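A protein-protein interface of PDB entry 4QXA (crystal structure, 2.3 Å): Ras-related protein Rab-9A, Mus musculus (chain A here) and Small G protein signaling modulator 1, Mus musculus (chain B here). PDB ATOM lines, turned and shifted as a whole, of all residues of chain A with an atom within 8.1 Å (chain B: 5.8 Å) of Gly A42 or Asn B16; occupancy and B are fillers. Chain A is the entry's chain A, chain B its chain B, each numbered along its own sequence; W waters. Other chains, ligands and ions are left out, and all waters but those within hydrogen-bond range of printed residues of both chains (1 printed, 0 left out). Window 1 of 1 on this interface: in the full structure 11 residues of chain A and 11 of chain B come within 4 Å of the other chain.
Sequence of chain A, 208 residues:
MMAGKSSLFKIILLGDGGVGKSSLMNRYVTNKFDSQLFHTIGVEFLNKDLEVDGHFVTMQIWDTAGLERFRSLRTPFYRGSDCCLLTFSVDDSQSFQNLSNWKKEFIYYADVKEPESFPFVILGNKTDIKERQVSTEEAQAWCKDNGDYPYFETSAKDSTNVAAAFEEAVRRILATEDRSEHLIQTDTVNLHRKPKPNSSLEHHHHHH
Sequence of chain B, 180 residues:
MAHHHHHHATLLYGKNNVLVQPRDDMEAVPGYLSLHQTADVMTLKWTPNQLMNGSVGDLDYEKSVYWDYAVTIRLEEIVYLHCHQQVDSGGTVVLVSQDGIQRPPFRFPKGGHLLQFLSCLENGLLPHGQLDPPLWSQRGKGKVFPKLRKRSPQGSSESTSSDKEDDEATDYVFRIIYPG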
ATOM      1  N   SER A  22     -25.916   9.483 -14.524  1.00  0.00           N
ATOM      2  CA  SER A  22     -24.960   8.392 -14.482  1.00  0.00           C
ATOM      3  C   SER A  22     -25.650   7.036 -14.521  1.00  0.00           C
ATOM      4  O   SER A  22     -25.166   6.099 -15.158  1.00  0.00           O
ATOM      5  CB  SER A  22     -24.098   8.487 -13.238  1.00  0.00           C
ATOM      6  OG  SER A  22     -23.051   9.388 -13.486  1.00  0.00           O
ATOM      7  N   PHE A  38     -23.590   9.116  -5.147  1.00  0.00           N
ATOM      8  CA  PHE A  38     -22.329   9.779  -5.435  1.00  0.00           C
ATOM      9  C   PHE A  38     -22.510  10.828  -6.526  1.00  0.00           C
ATOM     10  O   PHE A  38     -22.939  10.533  -7.646  1.00  0.00           O
ATOM     11  CB  PHE A  38     -21.224   8.797  -5.845  1.00  0.00           C
ATOM     12  CG  PHE A  38     -20.015   9.482  -6.421  1.00  0.00           C
ATOM     13  CD1 PHE A  38     -19.080  10.096  -5.577  1.00  0.00           C
ATOM     14  CD2 PHE A  38     -19.822   9.548  -7.806  1.00  0.00           C
ATOM     15  CE1 PHE A  38     -17.973  10.766  -6.102  1.00  0.00           C
ATOM     16  CE2 PHE A  38     -18.710  10.213  -8.355  1.00  0.00           C
ATOM     17  CZ  PHE A  38     -17.785  10.824  -7.504  1.00  0.00           C
ATOM     18  N   HIS A  39     -22.169  12.061  -6.196  1.00  0.00           N
ATOM     19  CA  HIS A  39     -22.216  13.129  -7.185  1.00  0.00           C
ATOM     20  C   HIS A  39     -21.007  13.018  -8.099  1.00  0.00           C
ATOM     21  O   HIS A  39     -19.885  12.988  -7.634  1.00  0.00           O
ATOM     22  CB  HIS A  39     -22.216  14.493  -6.474  1.00  0.00           C
ATOM     23  CG  HIS A  39     -23.514  14.825  -5.801  1.00  0.00           C
ATOM     24  ND1 HIS A  39     -24.717  14.843  -6.476  1.00  0.00           N
ATOM     25  CD2 HIS A  39     -23.796  15.176  -4.523  1.00  0.00           C
ATOM     26  CE1 HIS A  39     -25.681  15.201  -5.644  1.00  0.00           C
ATOM     27  NE2 HIS A  39     -25.149  15.407  -4.453  1.00  0.00           N
ATOM     28  N   THR A  40     -21.242  12.960  -9.392  1.00  0.00           N
ATOM     29  CA  THR A  40     -20.168  12.974 -10.365  1.00  0.00           C
ATOM     30  C   THR A  40     -19.412  14.273 -10.257  1.00  0.00           C
ATOM     31  O   THR A  40     -19.990  15.335 -10.176  1.00  0.00           O
ATOM     32  CB  THR A  40     -20.721  12.755 -11.767  1.00  0.00           C
ATOM     33  OG1 THR A  40     -21.122  11.407 -11.839  1.00  0.00           O
ATOM     34  CG2 THR A  40     -19.695  13.000 -12.866  1.00  0.00           C
ATOM     35  N   ILE A  41     -18.099  14.167 -10.221  1.00  0.00           N
ATOM     36  CA  ILE A  41     -17.290  15.346 -10.118  1.00  0.00           C
ATOM     37  C   ILE A  41     -16.749  15.609 -11.509  1.00  0.00           C
ATOM     38  O   ILE A  41     -17.190  16.524 -12.205  1.00  0.00           O
ATOM     39  CB  ILE A  41     -16.156  15.159  -9.084  1.00  0.00           C
ATOM     40  CG1 ILE A  41     -16.735  14.863  -7.686  1.00  0.00           C
ATOM     41  CG2 ILE A  41     -15.269  16.390  -9.063  1.00  0.00           C
ATOM     42  CD1 ILE A  41     -15.679  14.555  -6.587  1.00  0.00           C
ATOM     43  N   GLY A  42     -15.805  14.774 -11.922  1.00  0.00           N
ATOM     44  CA  GLY A  42     -15.230  14.891 -13.238  1.00  0.00           C
ATOM     45  C   GLY A  42     -16.062  14.146 -14.274  1.00  0.00           C
ATOM     46  O   GLY A  42     -16.776  13.189 -13.999  1.00  0.00           O
ATOM     47  N   VAL A  43     -15.935  14.611 -15.493  1.00  0.00           N
ATOM     48  CA  VAL A  43     -16.536  14.006 -16.676  1.00  0.00           C
ATOM     49  C   VAL A  43     -16.052  12.553 -16.999  1.00  0.00           C
ATOM     50  O   VAL A  43     -14.916  12.182 -16.696  1.00  0.00           O
ATOM     51  CB  VAL A  43     -16.241  14.968 -17.847  1.00  0.00           C
ATOM     52  CG1 VAL A  43     -15.309  14.343 -18.883  1.00  0.00           C
ATOM     53  CG2 VAL A  43     -17.517  15.540 -18.414  1.00  0.00           C
ATOM     54  N   GLU A  44     -16.933  11.741 -17.585  1.00  0.00           N
ATOM     55  CA  GLU A  44     -16.624  10.374 -18.010  1.00  0.00           C
ATOM     56  C   GLU A  44     -17.369  10.104 -19.303  1.00  0.00           C
ATOM     57  O   GLU A  44     -18.374  10.755 -19.592  1.00  0.00           O
ATOM     58  CB  GLU A  44     -17.089   9.331 -16.987  1.00  0.00           C
ATOM     59  CG  GLU A  44     -16.558   9.507 -15.588  1.00  0.00           C
ATOM     60  CD  GLU A  44     -16.984   8.373 -14.656  1.00  0.00           C
ATOM     61  OE1 GLU A  44     -16.636   8.408 -13.442  1.00  0.00           O
ATOM     62  OE2 GLU A  44     -17.665   7.443 -15.145  1.00  0.00           O
ATOM     63  N   PHE A  45     -16.892   9.145 -20.089  1.00  0.00           N
ATOM     64  CA  PHE A  45     -17.660   8.699 -21.252  1.00  0.00           C
ATOM     65  C   PHE A  45     -17.512   7.219 -21.504  1.00  0.00           C
ATOM     66  O   PHE A  45     -16.525   6.619 -21.089  1.00  0.00           O
ATOM     67  CB  PHE A  45     -17.341   9.502 -22.522  1.00  0.00           C
ATOM     68  CG  PHE A  45     -15.957   9.289 -23.057  1.00  0.00           C
ATOM     69  CD1 PHE A  45     -15.671   8.208 -23.878  1.00  0.00           C
ATOM     70  CD2 PHE A  45     -14.949  10.194 -22.769  1.00  0.00           C
ATOM     71  CE1 PHE A  45     -14.393   8.012 -24.381  1.00  0.00           C
ATOM     72  CE2 PHE A  45     -13.676  10.015 -23.271  1.00  0.00           C
ATOM     73  CZ  PHE A  45     -13.397   8.919 -24.078  1.00  0.00           C
ATOM     74  N   ASP A  63     -21.004  11.653 -19.688  1.00  0.00           N
ATOM     75  CA  ASP A  63     -21.645  11.877 -18.419  1.00  0.00           C
ATOM     76  C   ASP A  63     -20.994  13.082 -17.742  1.00  0.00           C
ATOM     77  O   ASP A  63     -19.772  13.245 -17.816  1.00  0.00           O
ATOM     78  CB  ASP A  63     -21.474  10.640 -17.567  1.00  0.00           C
ATOM     79  CG  ASP A  63     -22.272  10.698 -16.294  1.00  0.00           C
ATOM     80  OD1 ASP A  63     -23.271  11.474 -16.236  1.00  0.00           O
ATOM     81  OD2 ASP A  63     -21.890   9.956 -15.360  1.00  0.00           O
ATOM     82  N   THR A  64     -21.805  13.918 -17.084  1.00  0.00           N
ATOM     83  CA  THR A  64     -21.302  15.172 -16.515  1.00  0.00           C
ATOM     84  C   THR A  64     -21.778  15.411 -15.093  1.00  0.00           C
ATOM     85  O   THR A  64     -22.686  14.768 -14.609  1.00  0.00           O
ATOM     86  CB  THR A  64     -21.722  16.414 -17.367  1.00  0.00           C
ATOM     87  OG1 THR A  64     -23.142  16.551 -17.331  1.00  0.00           O
ATOM     88  CG2 THR A  64     -21.290  16.279 -18.824  1.00  0.00           C
ATOM     89  N   ALA A  65     -21.148  16.358 -14.423  1.00  0.00           N
ATOM     90  CA  ALA A  65     -21.586  16.782 -13.108  1.00  0.00           C
ATOM     91  C   ALA A  65     -22.861  17.644 -13.234  1.00  0.00           C
ATOM     92  O   ALA A  65     -22.905  18.579 -14.023  1.00  0.00           O
ATOM     93  CB  ALA A  65     -20.457  17.573 -12.412  1.00  0.00           C
ATOM     94  N   PHE A  70     -19.889  22.434  -9.927  1.00  0.00           N
ATOM     95  CA  PHE A  70     -18.961  21.670 -10.737  1.00  0.00           C
ATOM     96  C   PHE A  70     -19.016  22.097 -12.196  1.00  0.00           C
ATOM     97  O   PHE A  70     -18.517  21.396 -13.080  1.00  0.00           O
ATOM     98  CB  PHE A  70     -19.225  20.169 -10.616  1.00  0.00           C
ATOM     99  CG  PHE A  70     -18.841  19.583  -9.285  1.00  0.00           C
ATOM    100  CD1 PHE A  70     -17.764  20.079  -8.577  1.00  0.00           C
ATOM    101  CD2 PHE A  70     -19.558  18.531  -8.740  1.00  0.00           C
ATOM    102  CE1 PHE A  70     -17.414  19.541  -7.345  1.00  0.00           C
ATOM    103  CE2 PHE A  70     -19.208  17.987  -7.508  1.00  0.00           C
ATOM    104  CZ  PHE A  70     -18.135  18.504  -6.805  1.00  0.00           C
ATOM    105  N   LEU A  73     -16.142  21.980 -14.554  1.00  0.00           N
ATOM    106  CA  LEU A  73     -15.623  20.654 -14.880  1.00  0.00           C
ATOM    107  C   LEU A  73     -16.378  20.011 -16.041  1.00  0.00           C
ATOM    108  O   LEU A  73     -15.901  19.031 -16.599  1.00  0.00           O
ATOM    109  CB  LEU A  73     -15.610  19.715 -13.655  1.00  0.00           C
ATOM    110  CG  LEU A  73     -14.943  20.215 -12.359  1.00  0.00           C
ATOM    111  CD1 LEU A  73     -15.056  19.186 -11.256  1.00  0.00           C
ATOM    112  CD2 LEU A  73     -13.488  20.571 -12.628  1.00  0.00           C
ATOM    113  N   ARG A  74     -17.530  20.560 -16.430  1.00  0.00           N
ATOM    114  CA  ARG A  74     -18.294  19.957 -17.538  1.00  0.00           C
ATOM    115  C   ARG A  74     -18.288  20.794 -18.844  1.00  0.00           C
ATOM    116  O   ARG A  74     -18.198  20.251 -19.943  1.00  0.00           O
ATOM    117  CB  ARG A  74     -19.735  19.633 -17.098  1.00  0.00           C
ATOM    118  CG  ARG A  74     -20.530  20.876 -16.621  1.00  0.00           C
ATOM    119  CD  ARG A  74     -22.000  20.601 -16.259  1.00  0.00           C
ATOM    120  NE  ARG A  74     -22.663  21.842 -15.832  1.00  0.00           N
ATOM    121  CZ  ARG A  74     -22.969  22.163 -14.576  1.00  0.00           C
ATOM    122  NH1 ARG A  74     -22.730  21.312 -13.593  1.00  0.00           N
ATOM    123  NH2 ARG A  74     -23.540  23.336 -14.302  1.00  0.00           N
ATOM    124  N   PHE A  77     -16.446  20.408 -22.342  1.00  0.00           N
ATOM    125  CA  PHE A  77     -16.775  19.234 -23.133  1.00  0.00           C
ATOM    126  C   PHE A  77     -18.122  19.337 -23.858  1.00  0.00           C
ATOM    127  O   PHE A  77     -18.563  18.376 -24.474  1.00  0.00           O
ATOM    128  CB  PHE A  77     -16.710  18.007 -22.220  1.00  0.00           C
ATOM    129  CG  PHE A  77     -15.437  17.947 -21.423  1.00  0.00           C
ATOM    130  CD1 PHE A  77     -14.268  17.456 -21.998  1.00  0.00           C
ATOM    131  CD2 PHE A  77     -15.390  18.436 -20.130  1.00  0.00           C
ATOM    132  CE1 PHE A  77     -13.087  17.419 -21.278  1.00  0.00           C
ATOM    133  CE2 PHE A  77     -14.206  18.398 -19.398  1.00  0.00           C
ATOM    134  CZ  PHE A  77     -13.053  17.894 -19.977  1.00  0.00           C
ATOM    135  N   GLY B  14     -11.593   9.599 -18.562  1.00  0.00           N
ATOM    136  CA  GLY B  14     -11.808  10.223 -17.262  1.00  0.00           C
ATOM    137  C   GLY B  14     -12.565   9.235 -16.392  1.00  0.00           C
ATOM    138  O   GLY B  14     -13.477   8.564 -16.866  1.00  0.00           O
ATOM    139  N   LYS B  15     -12.184   9.117 -15.125  1.00  0.00           N
ATOM    140  CA  LYS B  15     -12.883   8.189 -14.230  1.00  0.00           C
ATOM    141  C   LYS B  15     -12.880   8.701 -12.803  1.00  0.00           C
ATOM    142  O   LYS B  15     -11.810   8.995 -12.255  1.00  0.00           O
ATOM    143  CB  LYS B  15     -12.241   6.805 -14.251  1.00  0.00           C
ATOM    144  CG  LYS B  15     -13.075   5.751 -13.527  1.00  0.00           C
ATOM    145  CD  LYS B  15     -14.412   5.503 -14.246  1.00  0.00           C
ATOM    146  CE  LYS B  15     -15.434   4.826 -13.325  1.00  0.00           C
ATOM    147  NZ  LYS B  15     -15.777   5.674 -12.121  1.00  0.00           N
ATOM    148  N   ASN B  16     -14.068   8.796 -12.207  1.00  0.00           N
ATOM    149  CA  ASN B  16     -14.205   9.234 -10.820  1.00  0.00           C
ATOM    150  C   ASN B  16     -13.947   8.091  -9.874  1.00  0.00           C
ATOM    151  O   ASN B  16     -14.139   6.930 -10.233  1.00  0.00           O
ATOM    152  CB  ASN B  16     -15.615   9.795 -10.532  1.00  0.00           C
ATOM    153  CG  ASN B  16     -15.857  11.156 -11.205  1.00  0.00           C
ATOM    154  OD1 ASN B  16     -15.490  12.194 -10.667  1.00  0.00           O
ATOM    155  ND2 ASN B  16     -16.476  11.141 -12.383  1.00  0.00           N
ATOM    156  N   ASN B  17     -13.520   8.438  -8.665  1.00  0.00           N
ATOM    157  CA  ASN B  17     -13.413   7.496  -7.560  1.00  0.00           C
ATOM    158  C   ASN B  17     -12.411   6.385  -7.801  1.00  0.00           C
ATOM    159  O   ASN B  17     -12.643   5.226  -7.431  1.00  0.00           O
ATOM    160  CB  ASN B  17     -14.784   6.924  -7.183  1.00  0.00           C
ATOM    161  CG  ASN B  17     -15.711   7.983  -6.580  1.00  0.00           C
ATOM    162  OD1 ASN B  17     -15.255   8.974  -6.000  1.00  0.00           O
ATOM    163  ND2 ASN B  17     -17.019   7.782  -6.730  1.00  0.00           N
ATOM    164  N   VAL B  18     -11.310   6.753  -8.447  1.00  0.00           N
ATOM    165  CA  VAL B  18     -10.111   5.922  -8.483  1.00  0.00           C
ATOM    166  C   VAL B  18      -9.391   6.177  -7.173  1.00  0.00           C
ATOM    167  O   VAL B  18      -9.075   7.321  -6.848  1.00  0.00           O
ATOM    168  CB  VAL B  18      -9.247   6.305  -9.681  1.00  0.00           C
ATOM    169  CG1 VAL B  18      -7.943   5.485  -9.718  1.00  0.00           C
ATOM    170  CG2 VAL B  18     -10.072   6.127 -10.962  1.00  0.00           C
ATOM    171  N   GLY B  31     -10.324   9.868  -5.965  1.00  0.00           N
ATOM    172  CA  GLY B  31      -9.811  10.909  -6.835  1.00  0.00           C
ATOM    173  C   GLY B  31     -10.238  10.682  -8.270  1.00  0.00           C
ATOM    174  O   GLY B  31     -10.834   9.667  -8.591  1.00  0.00           O
ATOM    175  N   TYR B  32      -9.927  11.634  -9.138  1.00  0.00           N
ATOM    176  CA  TYR B  32     -10.322  11.560 -10.548  1.00  0.00           C
ATOM    177  C   TYR B  32      -9.104  11.242 -11.415  1.00  0.00           C
ATOM    178  O   TYR B  32      -8.059  11.887 -11.319  1.00  0.00           O
ATOM    179  CB  TYR B  32     -10.925  12.902 -10.971  1.00  0.00           C
ATOM    180  CG  TYR B  32     -11.385  13.000 -12.407  1.00  0.00           C
ATOM    181  CD1 TYR B  32     -12.529  12.344 -12.834  1.00  0.00           C
ATOM    182  CD2 TYR B  32     -10.693  13.783 -13.326  1.00  0.00           C
ATOM    183  CE1 TYR B  32     -12.971  12.440 -14.145  1.00  0.00           C
ATOM    184  CE2 TYR B  32     -11.112  13.871 -14.644  1.00  0.00           C
ATOM    185  CZ  TYR B  32     -12.269  13.213 -15.039  1.00  0.00           C
ATOM    186  OH  TYR B  32     -12.722  13.322 -16.334  1.00  0.00           O
ATOM    187  N   LEU B  33      -9.242  10.234 -12.257  1.00  0.00           N
ATOM    188  CA  LEU B  33      -8.145   9.782 -13.086  1.00  0.00           C
ATOM    189  C   LEU B  33      -8.415  10.234 -14.503  1.00  0.00           C
ATOM    190  O   LEU B  33      -9.507  10.057 -15.012  1.00  0.00           O
ATOM    191  CB  LEU B  33      -8.032   8.253 -13.029  1.00  0.00           C
ATOM    192  CG  LEU B  33      -6.964   7.583 -13.893  1.00  0.00           C
ATOM    193  CD1 LEU B  33      -5.579   7.780 -13.285  1.00  0.00           C
ATOM    194  CD2 LEU B  33      -7.268   6.120 -14.006  1.00  0.00           C
ATOM    195  N   ASN B  49     -10.153  14.042  -4.727  1.00  0.00           N
ATOM    196  CA  ASN B  49     -11.435  14.731  -4.840  1.00  0.00           C
ATOM    197  C   ASN B  49     -11.526  16.114  -4.157  1.00  0.00           C
ATOM    198  O   ASN B  49     -12.116  17.037  -4.717  1.00  0.00           O
ATOM    199  CB  ASN B  49     -12.576  13.803  -4.435  1.00  0.00           C
ATOM    200  CG  ASN B  49     -12.859  12.765  -5.503  1.00  0.00           C
ATOM    201  OD1 ASN B  49     -12.362  12.878  -6.626  1.00  0.00           O
ATOM    202  ND2 ASN B  49     -13.657  11.761  -5.171  1.00  0.00           N
ATOM    203  N   PRO B 109     -13.075   1.498  -9.430  1.00  0.00           N
ATOM    204  CA  PRO B 109     -14.322   1.019  -8.825  1.00  0.00           C
ATOM    205  C   PRO B 109     -14.752  -0.279  -9.491  1.00  0.00           C
ATOM    206  O   PRO B 109     -14.317  -0.546 -10.620  1.00  0.00           O
ATOM    207  CB  PRO B 109     -15.333   2.127  -9.167  1.00  0.00           C
ATOM    208  CG  PRO B 109     -14.516   3.317  -9.544  1.00  0.00           C
ATOM    209  CD  PRO B 109     -13.268   2.761 -10.163  1.00  0.00           C
HETATM  210  O   HOH W   1     -14.181   8.147 -19.461  1.00  0.00           O
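The side-chain carboxylate (OE1) of Glu A44 lies within salt-bridge range of the side-chain amino group (NZ) of Lys B15.
N of Asn B16 lies within hydrogen-bond range of OE1 of Glu A44.
OH of Tyr B32 sits at hydrogen-bond distance from O of Val A43 (2.5 Å).
The side-chain amide oxygen (OD1) of Asn B16 is in hydrogen-bond range of the backbone NH (N) of Ile A41 (3.3 Å).
O of Gly A42 sits at hydrogen-bond distance from ND2 of Asn B16 (2.6 Å).
Water W1 bridges the backbone carbonyl oxygen of Gly B14 and the backbone NH of Phe A45.
Of the 10 printed residues of chain B, 6 touch a printed residue of chain A.
Hydrophobic or aromatic side chains of chain B that line the printed part of chain A: Tyr B32.
Along chain B the printed residues that touch a printed residue of chain A span positions 14 to 49.
Printed residues of chain A that touch a printed residue of chain B: Phe A38, Thr A40, Ile A41, Gly A42, Val A43 and Glu A44.
Among the printed residues, 12 pairs touch across the chains.
Asn B16 touches Phe A38 (CB to CE2, 3.8 Å).
Phe A38 touches Asn B17.
Thr A40 touches Asn B16.
Ile A41 touches Asn B49.
Gly A42 touches Tyr B32.
Val A43 touches Gly B14.
O of Gly B14 touches CG of Glu A44, 3.5 Å away.
Of the printed residues of chain B, Phe A38 touches Asn B16 and Asn B17.
Of the printed residues of chain B, Ile A41 touches Asn B16 (3.3 Å) and Asn B49 (3.5 Å).
Of chain B, only Asn B16 (2.6 Å) and Tyr B32 (3.5 Å) come within 4 Å of Gly A42.
Of the printed residues of chain A, Gly B14 touches Val A43 and Glu A44.
Printed residues of chain A within 4 Å of Lys B15: Glu A44.
Asn B16 touches just these residues of chain A: Phe A38 (3.8 Å), Thr A40 (3.7 Å), Ile A41 (3.3 Å), Gly A42 (2.6 Å) and Glu A44 (2.9 Å).
Of the printed residues of chain A, Asn B17 touches Phe A38.
Of the printed residues of chain A, Asn B49 touches Ile A41 (3.5 Å).
The nearest printed residue of chain B that does not touch Gly A42 is Lys B15 (6.1 Å).
The nearest residue of chain A that does not touch Asn B16 is Val A43 (4.7 Å).
O of Glu A44 is in hydrogen-bond range of N of Asp A63.
N of Asn B17 is in hydrogen-bond range of O of Gly B31.
The side-chain amide nitrogen of Asn B49 is in hydrogen-bond range of the side-chain amide oxygen of Asn B17 (3.3 Å).
N of Lys B15 is in hydrogen-bond range of O of Leu B33, at 2.8 Å.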
